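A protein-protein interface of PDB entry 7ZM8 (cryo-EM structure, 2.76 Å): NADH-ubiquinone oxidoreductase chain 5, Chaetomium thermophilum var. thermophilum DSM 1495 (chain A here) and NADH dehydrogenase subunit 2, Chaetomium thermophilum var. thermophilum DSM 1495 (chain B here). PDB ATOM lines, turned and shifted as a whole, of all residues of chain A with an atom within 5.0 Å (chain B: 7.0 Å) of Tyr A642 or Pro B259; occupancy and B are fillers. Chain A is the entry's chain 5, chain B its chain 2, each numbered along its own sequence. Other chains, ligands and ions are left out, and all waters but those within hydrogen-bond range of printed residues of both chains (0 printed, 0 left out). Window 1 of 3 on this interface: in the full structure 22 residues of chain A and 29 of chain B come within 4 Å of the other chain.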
ATOM      1  N   GLY A 638       9.474 -17.915   4.250  1.00  0.00           N
ATOM      2  CA  GLY A 638       8.074 -17.757   3.901  1.00  0.00           C
ATOM      3  C   GLY A 638       7.858 -17.044   2.590  1.00  0.00           C
ATOM      4  O   GLY A 638       6.800 -17.202   1.975  1.00  0.00           O
ATOM      5  N   PHE A 639       8.835 -16.245   2.156  1.00  0.00           N
ATOM      6  CA  PHE A 639       8.776 -15.651   0.826  1.00  0.00           C
ATOM      7  C   PHE A 639       8.970 -16.699  -0.260  1.00  0.00           C
ATOM      8  O   PHE A 639       8.212 -16.741  -1.231  1.00  0.00           O
ATOM      9  CB  PHE A 639       9.828 -14.551   0.712  1.00  0.00           C
ATOM     10  CG  PHE A 639       9.828 -13.842  -0.610  1.00  0.00           C
ATOM     11  CD1 PHE A 639       8.851 -12.912  -0.914  1.00  0.00           C
ATOM     12  CD2 PHE A 639      10.820 -14.098  -1.544  1.00  0.00           C
ATOM     13  CE1 PHE A 639       8.855 -12.254  -2.131  1.00  0.00           C
ATOM     14  CE2 PHE A 639      10.826 -13.446  -2.758  1.00  0.00           C
ATOM     15  CZ  PHE A 639       9.846 -12.522  -3.052  1.00  0.00           C
ATOM     16  N   ILE A 640       9.976 -17.561  -0.110  1.00  0.00           N
ATOM     17  CA  ILE A 640      10.276 -18.547  -1.142  1.00  0.00           C
ATOM     18  C   ILE A 640       9.133 -19.543  -1.293  1.00  0.00           C
ATOM     19  O   ILE A 640       8.795 -19.951  -2.411  1.00  0.00           O
ATOM     20  CB  ILE A 640      11.607 -19.255  -0.830  1.00  0.00           C
ATOM     21  CG1 ILE A 640      12.728 -18.235  -0.664  1.00  0.00           C
ATOM     22  CG2 ILE A 640      11.942 -20.279  -1.900  1.00  0.00           C
ATOM     23  CD1 ILE A 640      13.914 -18.761   0.107  1.00  0.00           C
ATOM     24  N   LEU A 641       8.531 -19.962  -0.180  1.00  0.00           N
ATOM     25  CA  LEU A 641       7.428 -20.915  -0.260  1.00  0.00           C
ATOM     26  C   LEU A 641       6.240 -20.337  -1.019  1.00  0.00           C
ATOM     27  O   LEU A 641       5.533 -21.067  -1.721  1.00  0.00           O
ATOM     28  CB  LEU A 641       7.007 -21.373   1.137  1.00  0.00           C
ATOM     29  CG  LEU A 641       7.800 -22.509   1.787  1.00  0.00           C
ATOM     30  CD1 LEU A 641       7.626 -23.775   0.964  1.00  0.00           C
ATOM     31  CD2 LEU A 641       9.269 -22.201   1.963  1.00  0.00           C
ATOM     32  N   TYR A 642       5.996 -19.034  -0.885  1.00  0.00           N
ATOM     33  CA  TYR A 642       4.940 -18.418  -1.681  1.00  0.00           C
ATOM     34  C   TYR A 642       5.319 -18.364  -3.154  1.00  0.00           C
ATOM     35  O   TYR A 642       4.466 -18.542  -4.028  1.00  0.00           O
ATOM     36  CB  TYR A 642       4.617 -17.021  -1.152  1.00  0.00           C
ATOM     37  CG  TYR A 642       3.686 -17.015   0.040  1.00  0.00           C
ATOM     38  CD1 TYR A 642       3.507 -18.146   0.812  1.00  0.00           C
ATOM     39  CD2 TYR A 642       2.986 -15.875   0.386  1.00  0.00           C
ATOM     40  CE1 TYR A 642       2.660 -18.139   1.894  1.00  0.00           C
ATOM     41  CE2 TYR A 642       2.135 -15.861   1.464  1.00  0.00           C
ATOM     42  CZ  TYR A 642       1.975 -16.991   2.212  1.00  0.00           C
ATOM     43  OH  TYR A 642       1.129 -16.980   3.290  1.00  0.00           O
ATOM     44  N   LEU A 643       6.597 -18.121  -3.445  1.00  0.00           N
ATOM     45  CA  LEU A 643       7.050 -18.057  -4.830  1.00  0.00           C
ATOM     46  C   LEU A 643       6.990 -19.419  -5.502  1.00  0.00           C
ATOM     47  O   LEU A 643       6.602 -19.524  -6.669  1.00  0.00           O
ATOM     48  CB  LEU A 643       8.467 -17.492  -4.893  1.00  0.00           C
ATOM     49  CG  LEU A 643       8.588 -15.977  -4.998  1.00  0.00           C
ATOM     50  CD1 LEU A 643       8.015 -15.553  -6.314  1.00  0.00           C
ATOM     51  CD2 LEU A 643       7.860 -15.271  -3.882  1.00  0.00           C
ATOM     52  N   ILE A 644       7.384 -20.471  -4.786  1.00  0.00           N
ATOM     53  CA  ILE A 644       7.318 -21.815  -5.347  1.00  0.00           C
ATOM     54  C   ILE A 644       5.875 -22.206  -5.628  1.00  0.00           C
ATOM     55  O   ILE A 644       5.557 -22.750  -6.690  1.00  0.00           O
ATOM     56  CB  ILE A 644       8.008 -22.816  -4.405  1.00  0.00           C
ATOM     57  CG1 ILE A 644       9.523 -22.629  -4.460  1.00  0.00           C
ATOM     58  CG2 ILE A 644       7.626 -24.238  -4.756  1.00  0.00           C
ATOM     59  CD1 ILE A 644      10.276 -23.444  -3.434  1.00  0.00           C
ATOM     60  N   TYR A 645       4.977 -21.922  -4.686  1.00  0.00           N
ATOM     61  CA  TYR A 645       3.594 -22.353  -4.828  1.00  0.00           C
ATOM     62  C   TYR A 645       2.914 -21.684  -6.014  1.00  0.00           C
ATOM     63  O   TYR A 645       2.132 -22.320  -6.731  1.00  0.00           O
ATOM     64  CB  TYR A 645       2.834 -22.069  -3.534  1.00  0.00           C
ATOM     65  CG  TYR A 645       1.344 -22.275  -3.628  1.00  0.00           C
ATOM     66  CD1 TYR A 645       0.777 -23.504  -3.330  1.00  0.00           C
ATOM     67  CD2 TYR A 645       0.502 -21.237  -3.992  1.00  0.00           C
ATOM     68  CE1 TYR A 645      -0.584 -23.698  -3.408  1.00  0.00           C
ATOM     69  CE2 TYR A 645      -0.858 -21.419  -4.074  1.00  0.00           C
ATOM     70  CZ  TYR A 645      -1.399 -22.650  -3.779  1.00  0.00           C
ATOM     71  OH  TYR A 645      -2.758 -22.832  -3.856  1.00  0.00           O
ATOM     72  N   ASN A 646       3.145 -20.401  -6.229  1.00  0.00           N
ATOM     73  CA  ASN A 646       2.423 -19.635  -7.279  1.00  0.00           C
ATOM     74  C   ASN A 646       3.262 -19.501  -8.550  1.00  0.00           C
ATOM     75  O   ASN A 646       2.966 -18.592  -9.340  1.00  0.00           O
ATOM     76  CB  ASN A 646       2.012 -18.265  -6.753  1.00  0.00           C
ATOM     77  CG  ASN A 646       0.640 -17.829  -7.213  1.00  0.00           C
ATOM     78  OD1 ASN A 646      -0.049 -18.566  -7.912  1.00  0.00           O
ATOM     79  ND2 ASN A 646       0.239 -16.631  -6.824  1.00  0.00           N
ATOM     80  N   LEU B 245       2.516 -10.447  -6.446  1.00  0.00           N
ATOM     81  CA  LEU B 245       2.790 -11.444  -5.419  1.00  0.00           C
ATOM     82  C   LEU B 245       3.905 -10.982  -4.486  1.00  0.00           C
ATOM     83  O   LEU B 245       3.760 -11.043  -3.263  1.00  0.00           O
ATOM     84  CB  LEU B 245       3.134 -12.774  -6.084  1.00  0.00           C
ATOM     85  CG  LEU B 245       3.516 -13.972  -5.219  1.00  0.00           C
ATOM     86  CD1 LEU B 245       2.317 -14.509  -4.479  1.00  0.00           C
ATOM     87  CD2 LEU B 245       4.136 -15.044  -6.083  1.00  0.00           C
ATOM     88  N   SER B 248       2.647  -8.213  -2.531  1.00  0.00           N
ATOM     89  CA  SER B 248       1.780  -8.625  -1.435  1.00  0.00           C
ATOM     90  C   SER B 248       2.562  -9.078  -0.208  1.00  0.00           C
ATOM     91  O   SER B 248       2.076  -8.920   0.914  1.00  0.00           O
ATOM     92  CB  SER B 248       0.842  -9.736  -1.898  1.00  0.00           C
ATOM     93  OG  SER B 248       1.556 -10.925  -2.170  1.00  0.00           O
ATOM     94  N   ILE B 249       3.757  -9.644  -0.392  1.00  0.00           N
ATOM     95  CA  ILE B 249       4.560 -10.080   0.750  1.00  0.00           C
ATOM     96  C   ILE B 249       4.922  -8.908   1.645  1.00  0.00           C
ATOM     97  O   ILE B 249       4.925  -9.031   2.877  1.00  0.00           O
ATOM     98  CB  ILE B 249       5.820 -10.839   0.286  1.00  0.00           C
ATOM     99  CG1 ILE B 249       5.520 -11.786  -0.878  1.00  0.00           C
ATOM    100  CG2 ILE B 249       6.458 -11.574   1.443  1.00  0.00           C
ATOM    101  CD1 ILE B 249       4.328 -12.703  -0.651  1.00  0.00           C
ATOM    102  N   LEU B 252       1.762  -7.980   3.487  1.00  0.00           N
ATOM    103  CA  LEU B 252       1.424  -9.040   4.431  1.00  0.00           C
ATOM    104  C   LEU B 252       2.248  -8.917   5.700  1.00  0.00           C
ATOM    105  O   LEU B 252       1.736  -9.123   6.803  1.00  0.00           O
ATOM    106  CB  LEU B 252       1.635 -10.411   3.793  1.00  0.00           C
ATOM    107  CG  LEU B 252       0.586 -10.920   2.804  1.00  0.00           C
ATOM    108  CD1 LEU B 252       1.084 -12.180   2.120  1.00  0.00           C
ATOM    109  CD2 LEU B 252      -0.760 -11.146   3.472  1.00  0.00           C
ATOM    110  N   SER B 256       1.108  -8.089   9.563  1.00  0.00           N
ATOM    111  CA  SER B 256       1.451  -9.231  10.409  1.00  0.00           C
ATOM    112  C   SER B 256       0.539 -10.426  10.147  1.00  0.00           C
ATOM    113  O   SER B 256      -0.053 -10.999  11.060  1.00  0.00           O
ATOM    114  CB  SER B 256       1.427  -8.846  11.883  1.00  0.00           C
ATOM    115  OG  SER B 256       1.730  -9.968  12.687  1.00  0.00           O
ATOM    116  N   ALA B 257       0.433 -10.799   8.882  1.00  0.00           N
ATOM    117  CA  ALA B 257      -0.247 -12.022   8.496  1.00  0.00           C
ATOM    118  C   ALA B 257       0.767 -13.155   8.452  1.00  0.00           C
ATOM    119  O   ALA B 257       1.850 -13.000   7.882  1.00  0.00           O
ATOM    120  CB  ALA B 257      -0.927 -11.857   7.139  1.00  0.00           C
ATOM    121  N   ALA B 258       0.413 -14.283   9.053  1.00  0.00           N
ATOM    122  CA  ALA B 258       1.294 -15.436   9.037  1.00  0.00           C
ATOM    123  C   ALA B 258       1.540 -15.876   7.596  1.00  0.00           C
ATOM    124  O   ALA B 258       0.626 -15.828   6.768  1.00  0.00           O
ATOM    125  CB  ALA B 258       0.689 -16.583   9.848  1.00  0.00           C
ATOM    126  N   PRO B 259       2.757 -16.323   7.261  1.00  0.00           N
ATOM    127  CA  PRO B 259       3.869 -16.607   8.173  1.00  0.00           C
ATOM    128  C   PRO B 259       4.759 -15.422   8.548  1.00  0.00           C
ATOM    129  O   PRO B 259       5.706 -15.614   9.296  1.00  0.00           O
ATOM    130  CB  PRO B 259       4.677 -17.629   7.386  1.00  0.00           C
ATOM    131  CG  PRO B 259       4.480 -17.220   5.980  1.00  0.00           C
ATOM    132  CD  PRO B 259       3.076 -16.720   5.880  1.00  0.00           C
ATOM    133  N   PHE B 260       4.466 -14.226   8.048  1.00  0.00           N
ATOM    134  CA  PHE B 260       5.314 -13.057   8.285  1.00  0.00           C
ATOM    135  C   PHE B 260       4.842 -12.285   9.517  1.00  0.00           C
ATOM    136  O   PHE B 260       4.589 -11.086   9.480  1.00  0.00           O
ATOM    137  CB  PHE B 260       5.333 -12.167   7.049  1.00  0.00           C
ATOM    138  CG  PHE B 260       5.393 -12.926   5.765  1.00  0.00           C
ATOM    139  CD1 PHE B 260       6.609 -13.337   5.245  1.00  0.00           C
ATOM    140  CD2 PHE B 260       4.236 -13.244   5.077  1.00  0.00           C
ATOM    141  CE1 PHE B 260       6.667 -14.041   4.064  1.00  0.00           C
ATOM    142  CE2 PHE B 260       4.291 -13.955   3.895  1.00  0.00           C
ATOM    143  CZ  PHE B 260       5.503 -14.348   3.388  1.00  0.00           C
ATOM    144  N   HIS B 261       4.749 -13.003  10.632  1.00  0.00           N
ATOM    145  CA  HIS B 261       4.070 -12.500  11.814  1.00  0.00           C
ATOM    146  C   HIS B 261       4.931 -12.438  13.067  1.00  0.00           C
ATOM    147  O   HIS B 261       4.485 -11.855  14.058  1.00  0.00           O
ATOM    148  CB  HIS B 261       2.841 -13.369  12.124  1.00  0.00           C
ATOM    149  CG  HIS B 261       3.191 -14.692  12.723  1.00  0.00           C
ATOM    150  ND1 HIS B 261       3.785 -15.701  11.999  1.00  0.00           N
ATOM    151  CD2 HIS B 261       3.064 -15.161  13.983  1.00  0.00           C
ATOM    152  CE1 HIS B 261       3.999 -16.738  12.783  1.00  0.00           C
ATOM    153  NE2 HIS B 261       3.576 -16.434  13.995  1.00  0.00           N
ATOM    154  N   PHE B 262       6.136 -13.009  13.063  1.00  0.00           N
ATOM    155  CA  PHE B 262       6.880 -13.212  14.302  1.00  0.00           C
ATOM    156  C   PHE B 262       7.249 -11.908  14.992  1.00  0.00           C
ATOM    157  O   PHE B 262       7.524 -11.913  16.195  1.00  0.00           O
ATOM    158  CB  PHE B 262       8.150 -14.019  14.030  1.00  0.00           C
ATOM    159  CG  PHE B 262       7.890 -15.430  13.599  1.00  0.00           C
ATOM    160  CD1 PHE B 262       7.554 -15.717  12.290  1.00  0.00           C
ATOM    161  CD2 PHE B 262       7.986 -16.474  14.502  1.00  0.00           C
ATOM    162  CE1 PHE B 262       7.318 -17.011  11.895  1.00  0.00           C
ATOM    163  CE2 PHE B 262       7.750 -17.770  14.107  1.00  0.00           C
ATOM    164  CZ  PHE B 262       7.416 -18.038  12.806  1.00  0.00           C
ATOM    165  N   TYR B 313      -3.982 -15.736  -4.238  1.00  0.00           N
ATOM    166  CA  TYR B 313      -3.760 -17.036  -3.555  1.00  0.00           C
ATOM    167  C   TYR B 313      -2.904 -16.875  -2.296  1.00  0.00           C
ATOM    168  O   TYR B 313      -3.174 -17.584  -1.334  1.00  0.00           O
ATOM    169  CB  TYR B 313      -3.088 -18.023  -4.505  1.00  0.00           C
ATOM    170  CG  TYR B 313      -3.906 -18.347  -5.724  1.00  0.00           C
ATOM    171  CD1 TYR B 313      -5.270 -18.121  -5.748  1.00  0.00           C
ATOM    172  CD2 TYR B 313      -3.316 -18.882  -6.853  1.00  0.00           C
ATOM    173  CE1 TYR B 313      -6.027 -18.400  -6.870  1.00  0.00           C
ATOM    174  CE2 TYR B 313      -4.060 -19.175  -7.980  1.00  0.00           C
ATOM    175  CZ  TYR B 313      -5.420 -18.935  -7.989  1.00  0.00           C
ATOM    176  OH  TYR B 313      -6.154 -19.228  -9.098  1.00  0.00           O
ATOM    177  N   ALA B 314      -1.895 -16.010  -2.312  1.00  0.00           N
ATOM    178  CA  ALA B 314      -1.026 -15.765  -1.146  1.00  0.00           C
ATOM    179  C   ALA B 314      -1.852 -15.237   0.020  1.00  0.00           C
ATOM    180  O   ALA B 314      -1.532 -15.581   1.155  1.00  0.00           O
ATOM    181  CB  ALA B 314       0.032 -14.776  -1.524  1.00  0.00           C
ATOM    182  N   LEU B 315      -2.818 -14.376  -0.255  1.00  0.00           N
ATOM    183  CA  LEU B 315      -3.756 -13.897   0.781  1.00  0.00           C
ATOM    184  C   LEU B 315      -4.618 -15.060   1.290  1.00  0.00           C
ATOM    185  O   LEU B 315      -4.989 -15.009   2.455  1.00  0.00           O
ATOM    186  CB  LEU B 315      -4.615 -12.776   0.180  1.00  0.00           C
ATOM    187  CG  LEU B 315      -3.893 -11.734  -0.669  1.00  0.00           C
ATOM    188  CD1 LEU B 315      -4.904 -10.899  -1.429  1.00  0.00           C
ATOM    189  CD2 LEU B 315      -3.018 -10.842   0.195  1.00  0.00           C
ATOM    190  N   LEU B 316      -5.026 -15.997   0.431  1.00  0.00           N
ATOM    191  CA  LEU B 316      -5.813 -17.190   0.847  1.00  0.00           C
ATOM    192  C   LEU B 316      -4.968 -18.144   1.697  1.00  0.00           C
ATOM    193  O   LEU B 316      -5.532 -18.818   2.561  1.00  0.00           O
ATOM    194  CB  LEU B 316      -6.396 -17.914  -0.362  1.00  0.00           C
ATOM    195  CG  LEU B 316      -7.869 -17.665  -0.650  1.00  0.00           C
ATOM    196  CD1 LEU B 316      -8.334 -18.599  -1.748  1.00  0.00           C
ATOM    197  CD2 LEU B 316      -8.707 -17.863   0.600  1.00  0.00           C
ATOM    198  N   ILE B 317      -3.667 -18.175   1.478  1.00  0.00           N
ATOM    199  CA  ILE B 317      -2.761 -19.085   2.227  1.00  0.00           C
ATOM    200  C   ILE B 317      -2.388 -18.347   3.508  1.00  0.00           C
ATOM    201  O   ILE B 317      -2.312 -18.989   4.531  1.00  0.00           O
ATOM    202  CB  ILE B 317      -1.531 -19.472   1.381  1.00  0.00           C
ATOM    203  CG1 ILE B 317      -1.919 -20.068   0.029  1.00  0.00           C
ATOM    204  CG2 ILE B 317      -0.614 -20.405   2.151  1.00  0.00           C
ATOM    205  CD1 ILE B 317      -0.754 -20.168  -0.912  1.00  0.00           C
ATOM    206  N   SER B 318      -2.180 -17.037   3.437  1.00  0.00           N
ATOM    207  CA  SER B 318      -1.930 -16.275   4.653  1.00  0.00           C
ATOM    208  C   SER B 318      -3.118 -16.348   5.591  1.00  0.00           C
ATOM    209  O   SER B 318      -2.951 -16.494   6.805  1.00  0.00           O
ATOM    210  CB  SER B 318      -1.612 -14.817   4.324  1.00  0.00           C
ATOM    211  OG  SER B 318      -0.278 -14.665   3.890  1.00  0.00           O
ATOM    212  N   SER B 319      -4.330 -16.242   5.045  1.00  0.00           N
ATOM    213  CA  SER B 319      -5.521 -16.331   5.876  1.00  0.00           C
ATOM    214  C   SER B 319      -5.612 -17.688   6.556  1.00  0.00           C
ATOM    215  O   SER B 319      -5.884 -17.770   7.757  1.00  0.00           O
ATOM    216  CB  SER B 319      -6.759 -16.064   5.032  1.00  0.00           C
ATOM    217  OG  SER B 319      -7.030 -17.159   4.181  1.00  0.00           O
ATOM    218  N   LEU B 321      -3.108 -19.721   7.188  1.00  0.00           N
ATOM    219  CA  LEU B 321      -2.028 -19.804   8.162  1.00  0.00           C
ATOM    220  C   LEU B 321      -2.262 -18.867   9.336  1.00  0.00           C
ATOM    221  O   LEU B 321      -1.885 -19.179  10.468  1.00  0.00           O
ATOM    222  CB  LEU B 321      -0.692 -19.501   7.487  1.00  0.00           C
ATOM    223  CG  LEU B 321      -0.176 -20.542   6.495  1.00  0.00           C
ATOM    224  CD1 LEU B 321       1.173 -20.133   5.953  1.00  0.00           C
ATOM    225  CD2 LEU B 321      -0.095 -21.911   7.133  1.00  0.00           C
ATOM    226  N   SER B 322      -2.875 -17.709   9.093  1.00  0.00           N
ATOM    227  CA  SER B 322      -3.115 -16.763  10.177  1.00  0.00           C
ATOM    228  C   SER B 322      -4.186 -17.273  11.130  1.00  0.00           C
ATOM    229  O   SER B 322      -4.098 -17.055  12.341  1.00  0.00           O
ATOM    230  CB  SER B 322      -3.506 -15.398   9.612  1.00  0.00           C
ATOM    231  OG  SER B 322      -2.567 -14.953   8.652  1.00  0.00           O
ATOM    232  N   ILE B 325      -2.177 -20.199  13.148  1.00  0.00           N
ATOM    233  CA  ILE B 325      -1.132 -19.691  14.032  1.00  0.00           C
ATOM    234  C   ILE B 325      -1.718 -18.786  15.105  1.00  0.00           C
ATOM    235  O   ILE B 325      -1.377 -18.901  16.286  1.00  0.00           O
ATOM    236  CB  ILE B 325      -0.041 -18.969  13.221  1.00  0.00           C
ATOM    237  CG1 ILE B 325       0.590 -19.921  12.201  1.00  0.00           C
ATOM    238  CG2 ILE B 325       1.006 -18.371  14.141  1.00  0.00           C
ATOM    239  CD1 ILE B 325       1.265 -21.118  12.821  1.00  0.00           C
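Phe B260 touches Gly A638 (CZ to O, 3.4 Å).
Phe A639 touches Ile B249 (CD1 to CG1, 3.5 Å).
Phe B260 touches Phe A639 (CE1 to N, 3.6 Å).
Tyr A642 touches Leu B252.
Ala B258 touches Tyr A642 (O to OH, 3.7 Å).
Ala B314 touches Tyr A642 (CB to CD2, 3.7 Å).
C of Ile B317 touches OH of Tyr A642 (3.8 Å).
Tyr A645 touches Ile B317.
Leu B245 touches Asn A646.
Asn A646 touches Tyr B313 (OD1 to CD2, 3.4 Å).
OG of Ser B318 sits at hydrogen-bond distance from OH of Tyr A642 (2.8 Å).
The backbone carbonyl oxygen (O) of Leu B245 is in hydrogen-bond range of the side-chain hydroxyl (OG) of Ser B248, 2.5 Å away.
The backbone carbonyl oxygen (O) of Leu B252 is in hydrogen-bond range of the backbone NH (N) of Ala B257.
O of Ala B258 lies within hydrogen-bond range of OG of Ser B318, at 3.2 Å.
N of Ala B258 lies within hydrogen-bond range of OG of Ser B322, at 3.1 Å.
O of Ala B314 lies within hydrogen-bond range of OG of Ser B318 (3.1 Å).
O of Ser B318 sits at hydrogen-bond distance from OG of Ser B322, at 2.4 Å.
Tyr A642 touches just these residues of chain B: Ile B249, Leu B252, Ala B258, Pro B259, Phe B260, Ala B314, Ile B317 and Ser B318.
Of chain A, only Tyr A642 comes within 4 Å of Pro B259.
Printed residues of chain A within 4 Å of Leu B252: Tyr A642.
Of the printed residues of chain A, Ala B314 touches Tyr A642 (3.7 Å).
Printed residues of chain A within 4 Å of Ile B317: Tyr A642 and Tyr A645.
Phe B262 touches none of the printed residues of chain A.
Ser B256 touches none of the printed residues of chain A.
The nearest residue of chain B that does not touch Tyr A642 is Leu B245 (4.1 Å).
The nearest residue of chain A that does not touch Pro B259 is Gly A638 (4.2 Å).
The nearest printed residue of chain B that does not touch Leu A643 is Ile B249 (5.2 Å).
Hydrophobic or aromatic side chains of chain B that line the printed part of chain A: Leu B245, Ile B249, Leu B252, Pro B259, Phe B260, Tyr B313, Ala B314 and Ile B317.
Of the 9 printed residues of chain A, 6 touch a printed residue of chain B.
Hydrophobic or aromatic side chains of chain A within 4 Å of the printed part of chain B: Phe A639, Tyr A642, Leu A643 and Tyr A645.
Among the printed residues, 15 pairs touch across the chains.
Among the printed residues, no Asp or Glu carboxylate lies within 4 Å of a Lys or Arg side-chain nitrogen of the other chain.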
